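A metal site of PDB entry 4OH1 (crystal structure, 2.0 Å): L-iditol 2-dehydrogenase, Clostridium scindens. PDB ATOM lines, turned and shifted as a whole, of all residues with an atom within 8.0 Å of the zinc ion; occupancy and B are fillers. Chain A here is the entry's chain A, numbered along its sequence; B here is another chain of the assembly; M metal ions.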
ATOM      1  N   LYS A 104     -23.167  -4.421 -26.927  1.00  0.00           N
ATOM      2  CA  LYS A 104     -22.257  -5.560 -26.917  1.00  0.00           C
ATOM      3  C   LYS A 104     -21.837  -5.915 -25.495  1.00  0.00           C
ATOM      4  O   LYS A 104     -21.096  -5.179 -24.843  1.00  0.00           O
ATOM      5  CB  LYS A 104     -21.019  -5.234 -27.743  1.00  0.00           C
ATOM      6  CG  LYS A 104     -19.963  -6.381 -27.821  1.00  0.00           C
ATOM      7  CD  LYS A 104     -20.571  -7.629 -28.353  1.00  0.00           C
ATOM      8  CE  LYS A 104     -19.564  -8.670 -28.711  1.00  0.00           C
ATOM      9  NZ  LYS A 104     -18.858  -9.102 -27.506  1.00  0.00           N
ATOM     10  N   TYR A 105     -22.282  -7.079 -25.031  1.00  0.00           N
ATOM     11  CA  TYR A 105     -21.946  -7.546 -23.698  1.00  0.00           C
ATOM     12  C   TYR A 105     -20.574  -8.262 -23.720  1.00  0.00           C
ATOM     13  O   TYR A 105     -20.264  -8.951 -24.679  1.00  0.00           O
ATOM     14  CB  TYR A 105     -23.034  -8.501 -23.221  1.00  0.00           C
ATOM     15  CG  TYR A 105     -24.413  -7.948 -23.468  1.00  0.00           C
ATOM     16  CD1 TYR A 105     -24.763  -6.676 -23.016  1.00  0.00           C
ATOM     17  CD2 TYR A 105     -25.364  -8.678 -24.179  1.00  0.00           C
ATOM     18  CE1 TYR A 105     -26.021  -6.125 -23.252  1.00  0.00           C
ATOM     19  CE2 TYR A 105     -26.653  -8.141 -24.422  1.00  0.00           C
ATOM     20  CZ  TYR A 105     -26.968  -6.860 -23.942  1.00  0.00           C
ATOM     21  OH  TYR A 105     -28.205  -6.290 -24.135  1.00  0.00           O
ATOM     22  N   CYS A 106     -19.769  -8.121 -22.676  1.00  0.00           N
ATOM     23  CA  CYS A 106     -18.427  -8.695 -22.707  1.00  0.00           C
ATOM     24  C   CYS A 106     -18.446 -10.167 -22.306  1.00  0.00           C
ATOM     25  O   CYS A 106     -17.505 -10.918 -22.608  1.00  0.00           O
ATOM     26  CB  CYS A 106     -17.500  -7.913 -21.766  1.00  0.00           C
ATOM     27  SG  CYS A 106     -17.675  -8.360 -20.049  1.00  0.00           S
ATOM     28  N   GLY A 107     -19.466 -10.584 -21.572  1.00  0.00           N
ATOM     29  CA  GLY A 107     -19.604 -11.994 -21.229  1.00  0.00           C
ATOM     30  C   GLY A 107     -18.577 -12.468 -20.244  1.00  0.00           C
ATOM     31  O   GLY A 107     -18.531 -13.655 -19.929  1.00  0.00           O
ATOM     32  N   CYS A 108     -17.769 -11.558 -19.690  1.00  0.00           N
ATOM     33  CA  CYS A 108     -16.786 -12.010 -18.730  1.00  0.00           C
ATOM     34  C   CYS A 108     -16.512 -11.067 -17.575  1.00  0.00           C
ATOM     35  O   CYS A 108     -15.484 -11.182 -16.942  1.00  0.00           O
ATOM     36  CB  CYS A 108     -15.471 -12.447 -19.423  1.00  0.00           C
ATOM     37  SG  CYS A 108     -14.690 -11.182 -20.371  1.00  0.00           S
ATOM     38  N   CYS A 109     -17.467 -10.208 -17.278  1.00  0.00           N
ATOM     39  CA  CYS A 109     -17.532  -9.456 -16.018  1.00  0.00           C
ATOM     40  C   CYS A 109     -18.626 -10.056 -15.081  1.00  0.00           C
ATOM     41  O   CYS A 109     -19.438 -10.966 -15.476  1.00  0.00           O
ATOM     42  CB  CYS A 109     -17.841  -7.961 -16.305  1.00  0.00           C
ATOM     43  SG  CYS A 109     -19.608  -7.632 -16.706  1.00  0.00           S
ATOM     44  N   GLU A 110     -18.685  -9.549 -13.841  1.00  0.00           N
ATOM     45  CA  GLU A 110     -19.560 -10.145 -12.849  1.00  0.00           C
ATOM     46  C   GLU A 110     -21.025  -9.909 -13.200  1.00  0.00           C
ATOM     47  O   GLU A 110     -21.859 -10.845 -13.131  1.00  0.00           O
ATOM     48  CB  GLU A 110     -19.264  -9.649 -11.442  1.00  0.00           C
ATOM     49  CG  GLU A 110     -20.186 -10.301 -10.445  1.00  0.00           C
ATOM     50  CD  GLU A 110     -19.817 -10.009  -9.004  1.00  0.00           C
ATOM     51  OE1 GLU A 110     -18.815 -10.590  -8.608  1.00  0.00           O
ATOM     52  OE2 GLU A 110     -20.516  -9.226  -8.290  1.00  0.00           O
ATOM     53  N   ASN A 111     -21.373  -8.692 -13.613  1.00  0.00           N
ATOM     54  CA  ASN A 111     -22.746  -8.493 -14.008  1.00  0.00           C
ATOM     55  C   ASN A 111     -23.192  -9.428 -15.158  1.00  0.00           C
ATOM     56  O   ASN A 111     -24.311 -10.003 -15.156  1.00  0.00           O
ATOM     57  CB  ASN A 111     -22.968  -7.034 -14.346  1.00  0.00           C
ATOM     58  CG  ASN A 111     -22.980  -6.163 -13.101  1.00  0.00           C
ATOM     59  OD1 ASN A 111     -23.413  -6.578 -12.048  1.00  0.00           O
ATOM     60  ND2 ASN A 111     -22.482  -4.974 -13.219  1.00  0.00           N
ATOM     61  N   CYS A 112     -22.302  -9.538 -16.147  1.00  0.00           N
ATOM     62  CA  CYS A 112     -22.563 -10.396 -17.271  1.00  0.00           C
ATOM     63  C   CYS A 112     -22.811 -11.773 -16.742  1.00  0.00           C
ATOM     64  O   CYS A 112     -23.791 -12.364 -17.085  1.00  0.00           O
ATOM     65  CB  CYS A 112     -21.396 -10.394 -18.279  1.00  0.00           C
ATOM     66  SG  CYS A 112     -21.660  -9.096 -19.536  1.00  0.00           S
ATOM     67  N   ARG A 113     -21.958 -12.278 -15.869  1.00  0.00           N
ATOM     68  CA  ARG A 113     -22.085 -13.671 -15.463  1.00  0.00           C
ATOM     69  C   ARG A 113     -23.066 -13.931 -14.304  1.00  0.00           C
ATOM     70  O   ARG A 113     -23.148 -15.062 -13.795  1.00  0.00           O
ATOM     71  CB  ARG A 113     -20.723 -14.231 -15.270  1.00  0.00           C
ATOM     72  CG  ARG A 113     -20.088 -14.304 -16.690  1.00  0.00           C
ATOM     73  CD  ARG A 113     -18.683 -14.695 -16.708  1.00  0.00           C
ATOM     74  NE  ARG A 113     -17.864 -14.054 -15.692  1.00  0.00           N
ATOM     75  CZ  ARG A 113     -16.574 -14.361 -15.517  1.00  0.00           C
ATOM     76  NH1 ARG A 113     -15.996 -15.261 -16.320  1.00  0.00           N
ATOM     77  NH2 ARG A 113     -15.872 -13.794 -14.552  1.00  0.00           N
ATOM     78  N   LYS A 116     -26.951 -10.212 -15.745  1.00  0.00           N
ATOM     79  CA  LYS A 116     -27.427  -8.848 -15.803  1.00  0.00           C
ATOM     80  C   LYS A 116     -26.617  -8.102 -16.866  1.00  0.00           C
ATOM     81  O   LYS A 116     -25.883  -7.176 -16.588  1.00  0.00           O
ATOM     82  CB  LYS A 116     -27.328  -8.229 -14.426  1.00  0.00           C
ATOM     83  CG  LYS A 116     -28.028  -9.069 -13.349  1.00  0.00           C
ATOM     84  CD  LYS A 116     -28.788  -8.200 -12.339  1.00  0.00           C
ATOM     85  CE  LYS A 116     -28.909  -8.834 -10.973  1.00  0.00           C
ATOM     86  NZ  LYS A 116     -27.569  -8.731 -10.349  1.00  0.00           N
ATOM     87  N   VAL A 117     -26.754  -8.536 -18.101  1.00  0.00           N
ATOM     88  CA  VAL A 117     -25.887  -8.058 -19.165  1.00  0.00           C
ATOM     89  C   VAL A 117     -26.152  -6.576 -19.476  1.00  0.00           C
ATOM     90  O   VAL A 117     -25.270  -5.897 -19.953  1.00  0.00           O
ATOM     91  CB  VAL A 117     -26.010  -8.945 -20.469  1.00  0.00           C
ATOM     92  CG1 VAL A 117     -25.365 -10.349 -20.306  1.00  0.00           C
ATOM     93  CG2 VAL A 117     -27.450  -9.087 -20.912  1.00  0.00           C
ATOM     94  N   ASN A 118     -27.368  -6.086 -19.231  1.00  0.00           N
ATOM     95  CA  ASN A 118     -27.669  -4.662 -19.326  1.00  0.00           C
ATOM     96  C   ASN A 118     -26.927  -3.763 -18.348  1.00  0.00           C
ATOM     97  O   ASN A 118     -26.946  -2.538 -18.515  1.00  0.00           O
ATOM     98  CB  ASN A 118     -29.163  -4.428 -19.174  1.00  0.00           C
ATOM     99  CG  ASN A 118     -29.680  -4.837 -17.769  1.00  0.00           C
ATOM    100  OD1 ASN A 118     -29.421  -5.964 -17.311  1.00  0.00           O
ATOM    101  ND2 ASN A 118     -30.367  -3.903 -17.093  1.00  0.00           N
ATOM    102  N   LEU A 119     -26.286  -4.384 -17.338  1.00  0.00           N
ATOM    103  CA  LEU A 119     -25.395  -3.711 -16.392  1.00  0.00           C
ATOM    104  C   LEU A 119     -23.964  -4.092 -16.688  1.00  0.00           C
ATOM    105  O   LEU A 119     -23.111  -3.957 -15.812  1.00  0.00           O
ATOM    106  CB  LEU A 119     -25.729  -4.072 -14.916  1.00  0.00           C
ATOM    107  CG  LEU A 119     -27.216  -3.991 -14.521  1.00  0.00           C
ATOM    108  CD1 LEU A 119     -27.415  -4.517 -13.112  1.00  0.00           C
ATOM    109  CD2 LEU A 119     -27.725  -2.551 -14.673  1.00  0.00           C
ATOM    110  N   CYS A 120     -23.676  -4.587 -17.877  1.00  0.00           N
ATOM    111  CA  CYS A 120     -22.291  -5.013 -18.217  1.00  0.00           C
ATOM    112  C   CYS A 120     -21.257  -3.940 -17.847  1.00  0.00           C
ATOM    113  O   CYS A 120     -21.409  -2.782 -18.234  1.00  0.00           O
ATOM    114  CB  CYS A 120     -22.138  -5.389 -19.732  1.00  0.00           C
ATOM    115  SG  CYS A 120     -20.391  -5.632 -20.211  1.00  0.00           S
ATOM    116  N   SER A 121     -20.197  -4.335 -17.134  1.00  0.00           N
ATOM    117  CA  SER A 121     -19.064  -3.396 -16.846  1.00  0.00           C
ATOM    118  C   SER A 121     -18.174  -2.967 -17.996  1.00  0.00           C
ATOM    119  O   SER A 121     -17.485  -1.985 -17.860  1.00  0.00           O
ATOM    120  CB  SER A 121     -18.079  -4.018 -15.865  1.00  0.00           C
ATOM    121  OG  SER A 121     -18.751  -4.371 -14.713  1.00  0.00           O
ATOM    122  N   ASN A 122     -18.067  -3.781 -19.035  1.00  0.00           N
ATOM    123  CA  ASN A 122     -17.255  -3.428 -20.202  1.00  0.00           C
ATOM    124  C   ASN A 122     -18.150  -3.272 -21.418  1.00  0.00           C
ATOM    125  O   ASN A 122     -17.852  -3.766 -22.511  1.00  0.00           O
ATOM    126  CB  ASN A 122     -16.234  -4.506 -20.492  1.00  0.00           C
ATOM    127  CG  ASN A 122     -15.411  -4.822 -19.300  1.00  0.00           C
ATOM    128  OD1 ASN A 122     -15.302  -5.966 -18.888  1.00  0.00           O
ATOM    129  ND2 ASN A 122     -14.886  -3.803 -18.689  1.00  0.00           N
ATOM    130  N   MET A 123     -19.226  -2.562 -21.208  1.00  0.00           N
ATOM    131  CA  MET A 123     -20.267  -2.465 -22.202  1.00  0.00           C
ATOM    132  C   MET A 123     -19.711  -1.851 -23.478  1.00  0.00           C
ATOM    133  O   MET A 123     -18.996  -0.881 -23.406  1.00  0.00           O
ATOM    134  CB  MET A 123     -21.389  -1.600 -21.645  1.00  0.00           C
ATOM    135  CG  MET A 123     -22.563  -1.465 -22.616  1.00  0.00           C
ATOM    136  SD  MET A 123     -23.667  -3.078 -22.655  1.00  0.00           S
ATOM    137  CE  MET A 123     -24.665  -2.639 -20.994  1.00  0.00           C
ATOM    138  N   GLY A 124     -19.990  -2.442 -24.631  1.00  0.00           N
ATOM    139  CA  GLY A 124     -19.661  -1.856 -25.938  1.00  0.00           C
ATOM    140  C   GLY A 124     -20.974  -1.357 -26.539  1.00  0.00           C
ATOM    141  O   GLY A 124     -22.043  -1.892 -26.211  1.00  0.00           O
ATOM    142  N   MET B  90      -9.092  -8.108 -20.708  1.00  0.00           N
ATOM    143  CA  MET B  90     -10.287  -8.132 -19.882  1.00  0.00           C
ATOM    144  C   MET B  90      -9.955  -8.267 -18.398  1.00  0.00           C
ATOM    145  O   MET B  90     -10.832  -8.514 -17.548  1.00  0.00           O
ATOM    146  CB  MET B  90     -11.193  -9.280 -20.296  1.00  0.00           C
ATOM    147  CG  MET B  90     -11.645  -9.167 -21.722  1.00  0.00           C
ATOM    148  SD  MET B  90     -13.035  -7.806 -21.968  1.00  0.00           S
ATOM    149  CE  MET B  90     -12.289  -6.987 -23.607  1.00  0.00           C
HETATM  150 ZN    ZN M   1     -19.741  -7.706 -19.075  1.00  0.00          ZN
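The backbone NH (N) of Gly 107 lies close to the side-chain sulfur (SG) of Cys 112 (3.3 Å).
The side-chain sulfur (SG) of Cys 120 lies close to the backbone NH (N) of Asn 122 (3.2 Å).
The side-chain sulfur (SG) of Cys 120 lies close to the backbone NH (N) of Met 123, 3.4 Å away.
The side-chain sulfur (SG) of Cys 109 lies close to the backbone NH (N) of Ser 121.
The side-chain sulfur (SG) of Cys 106 lies close to the side-chain amide oxygen (OD1) of Asn 122, 3.6 Å away.
The side-chain sulfur (SG) of Cys 109 lies close to the backbone NH (N) of Asn 111.
The backbone carbonyl oxygen (O) of Cys 109 lies within hydrogen-bond range of the guanidinium group (NE) of Arg 113.
The backbone carbonyl oxygen (O) of Cys 106 sits at hydrogen-bond distance from the side-chain sulfur (SG) of Cys 108.
Merely in contact with the zinc ion: Gly 107 and Ser 121.
Six residues have an atom within 4 Å of the zinc ion: Cys 106, Gly 107, Cys 109, Cys 112, Cys 120 and Ser 121.
The zinc ion is bound by SG of Cys 109 (2.4 Å), SG of Cys 106 (2.4 Å), SG of Cys 112 (2.4 Å) and SG of Cys 120 (2.5 Å).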
